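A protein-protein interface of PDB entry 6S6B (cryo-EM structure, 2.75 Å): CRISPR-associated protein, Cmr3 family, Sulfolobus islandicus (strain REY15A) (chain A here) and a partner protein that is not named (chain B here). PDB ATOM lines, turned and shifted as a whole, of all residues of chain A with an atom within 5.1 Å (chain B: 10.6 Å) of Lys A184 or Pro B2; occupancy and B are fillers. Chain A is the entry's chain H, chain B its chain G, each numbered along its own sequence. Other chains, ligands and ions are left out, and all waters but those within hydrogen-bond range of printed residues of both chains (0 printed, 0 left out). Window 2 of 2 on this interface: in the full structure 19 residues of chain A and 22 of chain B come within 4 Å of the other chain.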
ATOM      1  N   ILE A  49      27.911   5.622 -16.061  1.00  0.00           N
ATOM      2  CA  ILE A  49      27.199   6.536 -16.942  1.00  0.00           C
ATOM      3  C   ILE A  49      27.925   7.867 -17.009  1.00  0.00           C
ATOM      4  O   ILE A  49      28.147   8.425 -18.089  1.00  0.00           O
ATOM      5  CB  ILE A  49      25.754   6.728 -16.463  1.00  0.00           C
ATOM      6  CG1 ILE A  49      25.033   5.393 -16.385  1.00  0.00           C
ATOM      7  CG2 ILE A  49      25.023   7.663 -17.394  1.00  0.00           C
ATOM      8  CD1 ILE A  49      23.604   5.538 -15.974  1.00  0.00           C
ATOM      9  N   LYS A 180      20.133  13.312 -16.392  1.00  0.00           N
ATOM     10  CA  LYS A 180      21.230  12.543 -16.966  1.00  0.00           C
ATOM     11  C   LYS A 180      21.005  11.048 -16.767  1.00  0.00           C
ATOM     12  O   LYS A 180      20.926  10.290 -17.737  1.00  0.00           O
ATOM     13  CB  LYS A 180      22.561  12.990 -16.353  1.00  0.00           C
ATOM     14  CG  LYS A 180      22.823  14.474 -16.507  1.00  0.00           C
ATOM     15  CD  LYS A 180      24.306  14.769 -16.597  1.00  0.00           C
ATOM     16  CE  LYS A 180      24.972  14.677 -15.238  1.00  0.00           C
ATOM     17  NZ  LYS A 180      24.585  15.802 -14.346  1.00  0.00           N
ATOM     18  N   ILE A 181      20.891  10.612 -15.516  1.00  0.00           N
ATOM     19  CA  ILE A 181      20.590   9.205 -15.217  1.00  0.00           C
ATOM     20  C   ILE A 181      19.080   9.120 -15.016  1.00  0.00           C
ATOM     21  O   ILE A 181      18.550   9.188 -13.907  1.00  0.00           O
ATOM     22  CB  ILE A 181      21.391   8.688 -14.018  1.00  0.00           C
ATOM     23  CG1 ILE A 181      21.238   9.611 -12.811  1.00  0.00           C
ATOM     24  CG2 ILE A 181      22.853   8.608 -14.372  1.00  0.00           C
ATOM     25  CD1 ILE A 181      21.525   8.937 -11.494  1.00  0.00           C
ATOM     26  N   ASN A 182      18.367   8.950 -16.124  1.00  0.00           N
ATOM     27  CA  ASN A 182      16.928   8.733 -16.057  1.00  0.00           C
ATOM     28  C   ASN A 182      16.480   8.020 -17.317  1.00  0.00           C
ATOM     29  O   ASN A 182      16.874   8.405 -18.422  1.00  0.00           O
ATOM     30  CB  ASN A 182      16.162  10.046 -15.892  1.00  0.00           C
ATOM     31  CG  ASN A 182      14.745   9.827 -15.415  1.00  0.00           C
ATOM     32  OD1 ASN A 182      14.520   9.366 -14.300  1.00  0.00           O
ATOM     33  ND2 ASN A 182      13.779  10.154 -16.260  1.00  0.00           N
ATOM     34  N   GLY A 183      15.655   6.991 -17.148  1.00  0.00           N
ATOM     35  CA  GLY A 183      15.274   6.165 -18.272  1.00  0.00           C
ATOM     36  C   GLY A 183      16.429   5.437 -18.912  1.00  0.00           C
ATOM     37  O   GLY A 183      16.284   4.908 -20.015  1.00  0.00           O
ATOM     38  N   LYS A 184      17.574   5.390 -18.242  1.00  0.00           N
ATOM     39  CA  LYS A 184      18.782   4.814 -18.807  1.00  0.00           C
ATOM     40  C   LYS A 184      18.818   3.315 -18.565  1.00  0.00           C
ATOM     41  O   LYS A 184      18.496   2.841 -17.474  1.00  0.00           O
ATOM     42  CB  LYS A 184      20.020   5.464 -18.192  1.00  0.00           C
ATOM     43  CG  LYS A 184      20.081   6.956 -18.384  1.00  0.00           C
ATOM     44  CD  LYS A 184      20.214   7.317 -19.839  1.00  0.00           C
ATOM     45  CE  LYS A 184      21.578   6.928 -20.347  1.00  0.00           C
ATOM     46  NZ  LYS A 184      22.633   7.707 -19.652  1.00  0.00           N
ATOM     47  N   ILE A 185      19.201   2.575 -19.596  1.00  0.00           N
ATOM     48  CA  ILE A 185      19.445   1.145 -19.466  1.00  0.00           C
ATOM     49  C   ILE A 185      20.867   0.963 -18.962  1.00  0.00           C
ATOM     50  O   ILE A 185      21.824   1.387 -19.616  1.00  0.00           O
ATOM     51  CB  ILE A 185      19.235   0.423 -20.802  1.00  0.00           C
ATOM     52  CG1 ILE A 185      17.749   0.287 -21.100  1.00  0.00           C
ATOM     53  CG2 ILE A 185      19.885  -0.936 -20.776  1.00  0.00           C
ATOM     54  CD1 ILE A 185      17.034  -0.604 -20.139  1.00  0.00           C
ATOM     55  N   VAL A 186      21.010   0.347 -17.795  1.00  0.00           N
ATOM     56  CA  VAL A 186      22.319   0.170 -17.195  1.00  0.00           C
ATOM     57  C   VAL A 186      22.641  -1.310 -17.124  1.00  0.00           C
ATOM     58  O   VAL A 186      21.762  -2.172 -17.124  1.00  0.00           O
ATOM     59  CB  VAL A 186      22.415   0.799 -15.797  1.00  0.00           C
ATOM     60  CG1 VAL A 186      22.357   2.289 -15.904  1.00  0.00           C
ATOM     61  CG2 VAL A 186      21.299   0.288 -14.920  1.00  0.00           C
ATOM     62  N   ALA A 195      19.449  -3.533 -15.768  1.00  0.00           N
ATOM     63  CA  ALA A 195      18.397  -2.882 -15.008  1.00  0.00           C
ATOM     64  C   ALA A 195      18.094  -1.535 -15.645  1.00  0.00           C
ATOM     65  O   ALA A 195      18.854  -1.030 -16.472  1.00  0.00           O
ATOM     66  CB  ALA A 195      18.789  -2.702 -13.540  1.00  0.00           C
ATOM     67  N   LYS A 196      16.965  -0.953 -15.260  1.00  0.00           N
ATOM     68  CA  LYS A 196      16.548   0.347 -15.759  1.00  0.00           C
ATOM     69  C   LYS A 196      16.527   1.348 -14.616  1.00  0.00           C
ATOM     70  O   LYS A 196      16.190   1.000 -13.482  1.00  0.00           O
ATOM     71  CB  LYS A 196      15.171   0.276 -16.412  1.00  0.00           C
ATOM     72  CG  LYS A 196      14.771   1.549 -17.118  1.00  0.00           C
ATOM     73  CD  LYS A 196      13.415   1.420 -17.771  1.00  0.00           C
ATOM     74  CE  LYS A 196      12.388   0.881 -16.799  1.00  0.00           C
ATOM     75  NZ  LYS A 196      11.061   0.725 -17.444  1.00  0.00           N
ATOM     76  N   LEU A 197      16.888   2.589 -14.919  1.00  0.00           N
ATOM     77  CA  LEU A 197      16.958   3.648 -13.925  1.00  0.00           C
ATOM     78  C   LEU A 197      15.754   4.574 -14.038  1.00  0.00           C
ATOM     79  O   LEU A 197      15.205   4.787 -15.122  1.00  0.00           O
ATOM     80  CB  LEU A 197      18.246   4.452 -14.081  1.00  0.00           C
ATOM     81  CG  LEU A 197      19.481   3.738 -13.545  1.00  0.00           C
ATOM     82  CD1 LEU A 197      20.696   4.628 -13.642  1.00  0.00           C
ATOM     83  CD2 LEU A 197      19.247   3.318 -12.120  1.00  0.00           C
ATOM     84  N   PRO B   2      25.399   6.842 -23.175  1.00  0.00           N
ATOM     85  CA  PRO B   2      24.553   5.809 -22.573  1.00  0.00           C
ATOM     86  C   PRO B   2      25.177   4.426 -22.669  1.00  0.00           C
ATOM     87  O   PRO B   2      24.900   3.562 -21.838  1.00  0.00           O
ATOM     88  CB  PRO B   2      23.276   5.887 -23.402  1.00  0.00           C
ATOM     89  CG  PRO B   2      23.748   6.312 -24.750  1.00  0.00           C
ATOM     90  CD  PRO B   2      24.935   7.216 -24.522  1.00  0.00           C
ATOM     91  N   TYR B   3      26.013   4.229 -23.688  1.00  0.00           N
ATOM     92  CA  TYR B   3      26.667   2.950 -23.947  1.00  0.00           C
ATOM     93  C   TYR B   3      25.657   1.816 -24.087  1.00  0.00           C
ATOM     94  O   TYR B   3      25.968   0.655 -23.826  1.00  0.00           O
ATOM     95  CB  TYR B   3      27.707   2.639 -22.867  1.00  0.00           C
ATOM     96  CG  TYR B   3      28.768   3.708 -22.765  1.00  0.00           C
ATOM     97  CD1 TYR B   3      29.796   3.778 -23.693  1.00  0.00           C
ATOM     98  CD2 TYR B   3      28.730   4.662 -21.756  1.00  0.00           C
ATOM     99  CE1 TYR B   3      30.765   4.759 -23.613  1.00  0.00           C
ATOM    100  CE2 TYR B   3      29.697   5.647 -21.665  1.00  0.00           C
ATOM    101  CZ  TYR B   3      30.711   5.691 -22.599  1.00  0.00           C
ATOM    102  OH  TYR B   3      31.679   6.668 -22.522  1.00  0.00           O
ATOM    103  N   TYR B   4      24.427   2.157 -24.456  1.00  0.00           N
ATOM    104  CA  TYR B   4      23.456   1.227 -25.025  1.00  0.00           C
ATOM    105  C   TYR B   4      22.758   1.890 -26.200  1.00  0.00           C
ATOM    106  O   TYR B   4      21.531   1.967 -26.265  1.00  0.00           O
ATOM    107  CB  TYR B   4      22.464   0.704 -23.994  1.00  0.00           C
ATOM    108  CG  TYR B   4      23.033  -0.436 -23.195  1.00  0.00           C
ATOM    109  CD1 TYR B   4      23.172  -1.684 -23.766  1.00  0.00           C
ATOM    110  CD2 TYR B   4      23.422  -0.276 -21.880  1.00  0.00           C
ATOM    111  CE1 TYR B   4      23.695  -2.739 -23.062  1.00  0.00           C
ATOM    112  CE2 TYR B   4      23.941  -1.333 -21.163  1.00  0.00           C
ATOM    113  CZ  TYR B   4      24.074  -2.562 -21.763  1.00  0.00           C
ATOM    114  OH  TYR B   4      24.593  -3.624 -21.068  1.00  0.00           O
ATOM    115  N   ALA B   5      23.566   2.416 -27.124  1.00  0.00           N
ATOM    116  CA  ALA B   5      23.086   3.191 -28.265  1.00  0.00           C
ATOM    117  C   ALA B   5      21.797   2.653 -28.869  1.00  0.00           C
ATOM    118  O   ALA B   5      20.875   3.419 -29.166  1.00  0.00           O
ATOM    119  CB  ALA B   5      24.177   3.247 -29.333  1.00  0.00           C
ATOM    120  N   PHE B   6      21.707   1.340 -29.059  1.00  0.00           N
ATOM    121  CA  PHE B   6      20.536   0.758 -29.692  1.00  0.00           C
ATOM    122  C   PHE B   6      20.167  -0.549 -29.009  1.00  0.00           C
ATOM    123  O   PHE B   6      20.941  -1.121 -28.239  1.00  0.00           O
ATOM    124  CB  PHE B   6      20.762   0.527 -31.189  1.00  0.00           C
ATOM    125  CG  PHE B   6      21.956  -0.320 -31.495  1.00  0.00           C
ATOM    126  CD1 PHE B   6      21.871  -1.701 -31.455  1.00  0.00           C
ATOM    127  CD2 PHE B   6      23.164   0.263 -31.826  1.00  0.00           C
ATOM    128  CE1 PHE B   6      22.965  -2.481 -31.737  1.00  0.00           C
ATOM    129  CE2 PHE B   6      24.261  -0.511 -32.111  1.00  0.00           C
ATOM    130  CZ  PHE B   6      24.163  -1.887 -32.067  1.00  0.00           C
ATOM    131  N   ALA B   7      18.959  -1.013 -29.312  1.00  0.00           N
ATOM    132  CA  ALA B   7      18.439  -2.277 -28.818  1.00  0.00           C
ATOM    133  C   ALA B   7      17.620  -2.907 -29.927  1.00  0.00           C
ATOM    134  O   ALA B   7      16.820  -2.226 -30.572  1.00  0.00           O
ATOM    135  CB  ALA B   7      17.579  -2.088 -27.567  1.00  0.00           C
ATOM    136  N   LEU B  83      30.418  -6.003 -26.059  1.00  0.00           N
ATOM    137  CA  LEU B  83      29.643  -4.878 -26.552  1.00  0.00           C
ATOM    138  C   LEU B  83      28.168  -5.188 -26.723  1.00  0.00           C
ATOM    139  O   LEU B  83      27.381  -4.261 -26.928  1.00  0.00           O
ATOM    140  CB  LEU B  83      30.205  -4.392 -27.894  1.00  0.00           C
ATOM    141  CG  LEU B  83      31.572  -3.720 -27.846  1.00  0.00           C
ATOM    142  CD1 LEU B  83      32.070  -3.469 -29.251  1.00  0.00           C
ATOM    143  CD2 LEU B  83      31.498  -2.425 -27.063  1.00  0.00           C
ATOM    144  N   THR B  85      24.624  -7.455 -25.353  1.00  0.00           N
ATOM    145  CA  THR B  85      23.990  -8.204 -24.283  1.00  0.00           C
ATOM    146  C   THR B  85      22.657  -8.745 -24.764  1.00  0.00           C
ATOM    147  O   THR B  85      21.881  -8.031 -25.403  1.00  0.00           O
ATOM    148  CB  THR B  85      23.768  -7.338 -23.045  1.00  0.00           C
ATOM    149  OG1 THR B  85      24.944  -6.568 -22.784  1.00  0.00           O
ATOM    150  CG2 THR B  85      23.463  -8.200 -21.843  1.00  0.00           C
ATOM    151  N   LEU B 123       7.530  -4.806 -19.885  1.00  0.00           N
ATOM    152  CA  LEU B 123       8.692  -4.334 -19.141  1.00  0.00           C
ATOM    153  C   LEU B 123       9.912  -4.218 -20.043  1.00  0.00           C
ATOM    154  O   LEU B 123      10.641  -3.222 -19.998  1.00  0.00           O
ATOM    155  CB  LEU B 123       8.969  -5.276 -17.974  1.00  0.00           C
ATOM    156  CG  LEU B 123      10.263  -5.017 -17.212  1.00  0.00           C
ATOM    157  CD1 LEU B 123      10.250  -3.619 -16.649  1.00  0.00           C
ATOM    158  CD2 LEU B 123      10.448  -6.040 -16.108  1.00  0.00           C
ATOM    159  N   ASP B 126       9.105  -1.130 -22.621  1.00  0.00           N
ATOM    160  CA  ASP B 126       9.290   0.206 -22.069  1.00  0.00           C
ATOM    161  C   ASP B 126      10.764   0.519 -21.887  1.00  0.00           C
ATOM    162  O   ASP B 126      11.215   1.630 -22.184  1.00  0.00           O
ATOM    163  CB  ASP B 126       8.567   0.328 -20.731  1.00  0.00           C
ATOM    164  CG  ASP B 126       7.130  -0.120 -20.805  1.00  0.00           C
ATOM    165  OD1 ASP B 126       6.485   0.124 -21.845  1.00  0.00           O
ATOM    166  OD2 ASP B 126       6.644  -0.715 -19.822  1.00  0.00           O
ATOM    167  N   SER B 127      11.531  -0.457 -21.406  1.00  0.00           N
ATOM    168  CA  SER B 127      12.891  -0.197 -20.967  1.00  0.00           C
ATOM    169  C   SER B 127      13.794   0.265 -22.096  1.00  0.00           C
ATOM    170  O   SER B 127      14.778   0.960 -21.838  1.00  0.00           O
ATOM    171  CB  SER B 127      13.462  -1.447 -20.315  1.00  0.00           C
ATOM    172  OG  SER B 127      12.704  -1.795 -19.172  1.00  0.00           O
ATOM    173  N   ILE B 128      13.486  -0.090 -23.338  1.00  0.00           N
ATOM    174  CA  ILE B 128      14.339   0.276 -24.462  1.00  0.00           C
ATOM    175  C   ILE B 128      13.715   1.326 -25.359  1.00  0.00           C
ATOM    176  O   ILE B 128      14.359   1.744 -26.332  1.00  0.00           O
ATOM    177  CB  ILE B 128      14.736  -0.958 -25.293  1.00  0.00           C
ATOM    178  CG1 ILE B 128      13.526  -1.491 -26.044  1.00  0.00           C
ATOM    179  CG2 ILE B 128      15.300  -2.034 -24.391  1.00  0.00           C
ATOM    180  CD1 ILE B 128      13.779  -2.791 -26.757  1.00  0.00           C
ATOM    181  N   SER B 129      12.493   1.769 -25.070  1.00  0.00           N
ATOM    182  CA  SER B 129      11.885   2.830 -25.861  1.00  0.00           C
ATOM    183  C   SER B 129      12.671   4.129 -25.762  1.00  0.00           C
ATOM    184  O   SER B 129      12.614   4.959 -26.675  1.00  0.00           O
ATOM    185  CB  SER B 129      10.447   3.055 -25.407  1.00  0.00           C
ATOM    186  OG  SER B 129      10.404   3.352 -24.025  1.00  0.00           O
ATOM    187  N   GLN B 130      13.411   4.324 -24.670  1.00  0.00           N
ATOM    188  CA  GLN B 130      14.093   5.595 -24.466  1.00  0.00           C
ATOM    189  C   GLN B 130      15.351   5.712 -25.315  1.00  0.00           C
ATOM    190  O   GLN B 130      15.836   6.823 -25.545  1.00  0.00           O
ATOM    191  CB  GLN B 130      14.433   5.777 -22.990  1.00  0.00           C
ATOM    192  CG  GLN B 130      13.227   5.717 -22.065  1.00  0.00           C
ATOM    193  CD  GLN B 130      12.121   6.670 -22.477  1.00  0.00           C
ATOM    194  OE1 GLN B 130      10.951   6.293 -22.526  1.00  0.00           O
ATOM    195  NE2 GLN B 130      12.486   7.912 -22.775  1.00  0.00           N
ATOM    196  N   LEU B 131      15.899   4.591 -25.777  1.00  0.00           N
ATOM    197  CA  LEU B 131      17.076   4.621 -26.629  1.00  0.00           C
ATOM    198  C   LEU B 131      16.787   4.217 -28.062  1.00  0.00           C
ATOM    199  O   LEU B 131      17.528   4.622 -28.966  1.00  0.00           O
ATOM    200  CB  LEU B 131      18.175   3.713 -26.056  1.00  0.00           C
ATOM    201  CG  LEU B 131      17.849   2.244 -25.795  1.00  0.00           C
ATOM    202  CD1 LEU B 131      18.091   1.415 -27.025  1.00  0.00           C
ATOM    203  CD2 LEU B 131      18.677   1.717 -24.642  1.00  0.00           C
ATOM    204  N   SER B 132      15.741   3.432 -28.294  1.00  0.00           N
ATOM    205  CA  SER B 132      15.341   3.030 -29.641  1.00  0.00           C
ATOM    206  C   SER B 132      14.662   4.217 -30.305  1.00  0.00           C
ATOM    207  O   SER B 132      13.454   4.421 -30.174  1.00  0.00           O
ATOM    208  CB  SER B 132      14.412   1.827 -29.588  1.00  0.00           C
ATOM    209  OG  SER B 132      13.105   2.226 -29.217  1.00  0.00           O
ATOM    210  N   ASN B 133      15.445   5.006 -31.040  1.00  0.00           N
ATOM    211  CA  ASN B 133      14.875   6.074 -31.852  1.00  0.00           C
ATOM    212  C   ASN B 133      14.216   5.536 -33.115  1.00  0.00           C
ATOM    213  O   ASN B 133      13.917   6.305 -34.036  1.00  0.00           O
ATOM    214  CB  ASN B 133      15.943   7.110 -32.204  1.00  0.00           C
ATOM    215  CG  ASN B 133      15.351   8.477 -32.491  1.00  0.00           C
ATOM    216  OD1 ASN B 133      14.133   8.653 -32.480  1.00  0.00           O
ATOM    217  ND2 ASN B 133      16.212   9.456 -32.738  1.00  0.00           N
ATOM    218  N   LEU B 243      20.896  -5.914 -26.663  1.00  0.00           N
ATOM    219  CA  LEU B 243      21.342  -4.564 -26.372  1.00  0.00           C
ATOM    220  C   LEU B 243      22.784  -4.385 -26.811  1.00  0.00           C
ATOM    221  O   LEU B 243      23.639  -5.230 -26.536  1.00  0.00           O
ATOM    222  CB  LEU B 243      21.216  -4.273 -24.882  1.00  0.00           C
ATOM    223  CG  LEU B 243      19.825  -4.415 -24.293  1.00  0.00           C
ATOM    224  CD1 LEU B 243      19.932  -4.778 -22.840  1.00  0.00           C
ATOM    225  CD2 LEU B 243      19.093  -3.116 -24.458  1.00  0.00           C
ATOM    226  N   GLY B 244      23.054  -3.276 -27.484  1.00  0.00           N
ATOM    227  CA  GLY B 244      24.385  -3.039 -27.997  1.00  0.00           C
ATOM    228  C   GLY B 244      24.987  -1.731 -27.537  1.00  0.00           C
ATOM    229  O   GLY B 244      24.340  -0.683 -27.603  1.00  0.00           O
ATOM    230  N   LYS B 245      26.224  -1.782 -27.059  1.00  0.00           N
ATOM    231  CA  LYS B 245      26.933  -0.560 -26.735  1.00  0.00           C
ATOM    232  C   LYS B 245      27.360   0.147 -28.013  1.00  0.00           C
ATOM    233  O   LYS B 245      27.395  -0.438 -29.097  1.00  0.00           O
ATOM    234  CB  LYS B 245      28.147  -0.857 -25.860  1.00  0.00           C
ATOM    235  CG  LYS B 245      27.812  -1.635 -24.608  1.00  0.00           C
ATOM    236  CD  LYS B 245      28.748  -1.280 -23.481  1.00  0.00           C
ATOM    237  CE  LYS B 245      28.512  -2.170 -22.284  1.00  0.00           C
ATOM    238  NZ  LYS B 245      29.751  -2.887 -21.889  1.00  0.00           N
ATOM    239  N   GLU B 246      27.688   1.427 -27.877  1.00  0.00           N
ATOM    240  CA  GLU B 246      28.040   2.240 -29.031  1.00  0.00           C
ATOM    241  C   GLU B 246      29.467   1.934 -29.460  1.00  0.00           C
ATOM    242  O   GLU B 246      30.414   2.163 -28.699  1.00  0.00           O
ATOM    243  CB  GLU B 246      27.879   3.722 -28.709  1.00  0.00           C
ATOM    244  CG  GLU B 246      28.420   4.646 -29.784  1.00  0.00           C
ATOM    245  CD  GLU B 246      27.911   4.299 -31.171  1.00  0.00           C
ATOM    246  OE1 GLU B 246      26.732   3.911 -31.300  1.00  0.00           O
ATOM    247  OE2 GLU B 246      28.695   4.415 -32.136  1.00  0.00           O
ATOM    248  N   SER B 247      29.622   1.426 -30.676  1.00  0.00           N
ATOM    249  CA  SER B 247      30.934   1.094 -31.211  1.00  0.00           C
ATOM    250  C   SER B 247      30.818   0.956 -32.720  1.00  0.00           C
ATOM    251  O   SER B 247      29.728   1.040 -33.290  1.00  0.00           O
ATOM    252  CB  SER B 247      31.482  -0.185 -30.582  1.00  0.00           C
ATOM    253  OG  SER B 247      32.591  -0.664 -31.316  1.00  0.00           O
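Printed residues of chain B that touch a printed residue of chain A: Pro B2, Tyr B4, Ser B127, Gln B130 and Leu B131. Along chain B the printed residues that touch a printed residue of chain A span positions 2 to 131. Of the 11 printed residues of chain A, 4 touch a printed residue of chain B. Hydrophobic or aromatic side chains of chain A that line the printed part of chain B: Ile A185. Among the printed residues, 6 pairs touch across the chains. Among the printed residues, no Asp or Glu carboxylate lies within 4 Å of a Lys or Arg side-chain nitrogen of the other chain.
No residue of chain B comes within 4 Å of Asn A182. Gly A183 touches just one residue of chain B: Gln B130 (3.6 Å). Lys A184 touches just one residue of chain B: Pro B2. No residue of chain B comes within 4 Å of Val A186. Pro B2 touches one residue of chain A. Of the printed residues of chain A, Tyr B4 touches Ile A185. Leu B83 touches none of the printed residues of chain A. Of the printed residues of chain A, Ser B127 touches Ile A185 and Lys A196. Printed residues of chain A within 4 Å of Gln B130: Gly A183. Printed residues of chain A within 4 Å of Leu B131: Ile A185. Ser B132 touches none of the printed residues of chain A. The nearest printed residue of chain B that does not touch Lys A184 is Gln B130 (5.7 Å). The nearest residue of chain A that does not touch Pro B2 is Ile A185 (4.4 Å). The nearest printed residue of chain B that does not touch Lys A196 is Asp B126 (4.1 Å).
N of Leu A197 is in hydrogen-bond range of O of Lys A184, at 3.0 Å. The side-chain hydroxyl (OH) of Tyr B4 sits at hydrogen-bond distance from the side-chain hydroxyl (OG1) of Thr B85, 3.4 Å away. The side-chain hydroxyl of Ser B129 sits at hydrogen-bond distance from the side-chain amide oxygen of Gln B130, 3.3 Å away. O of Leu B123 sits at hydrogen-bond distance from OG of Ser B127, 2.6 Å away. O of Leu A197 lies within hydrogen-bond range of N of Gly A183 (3.0 Å).
NZ of Lys A196 lies within hydrogen-bond range of OG of Ser B127, 3.5 Å away.
Among the printed residues, merely in contact across the chains: Ile A185 with Ser B127, Ile A185 with Tyr B4, Gly A183 with Gln B130, Lys A184 with Pro B2 and Ile A185 with Leu B131.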
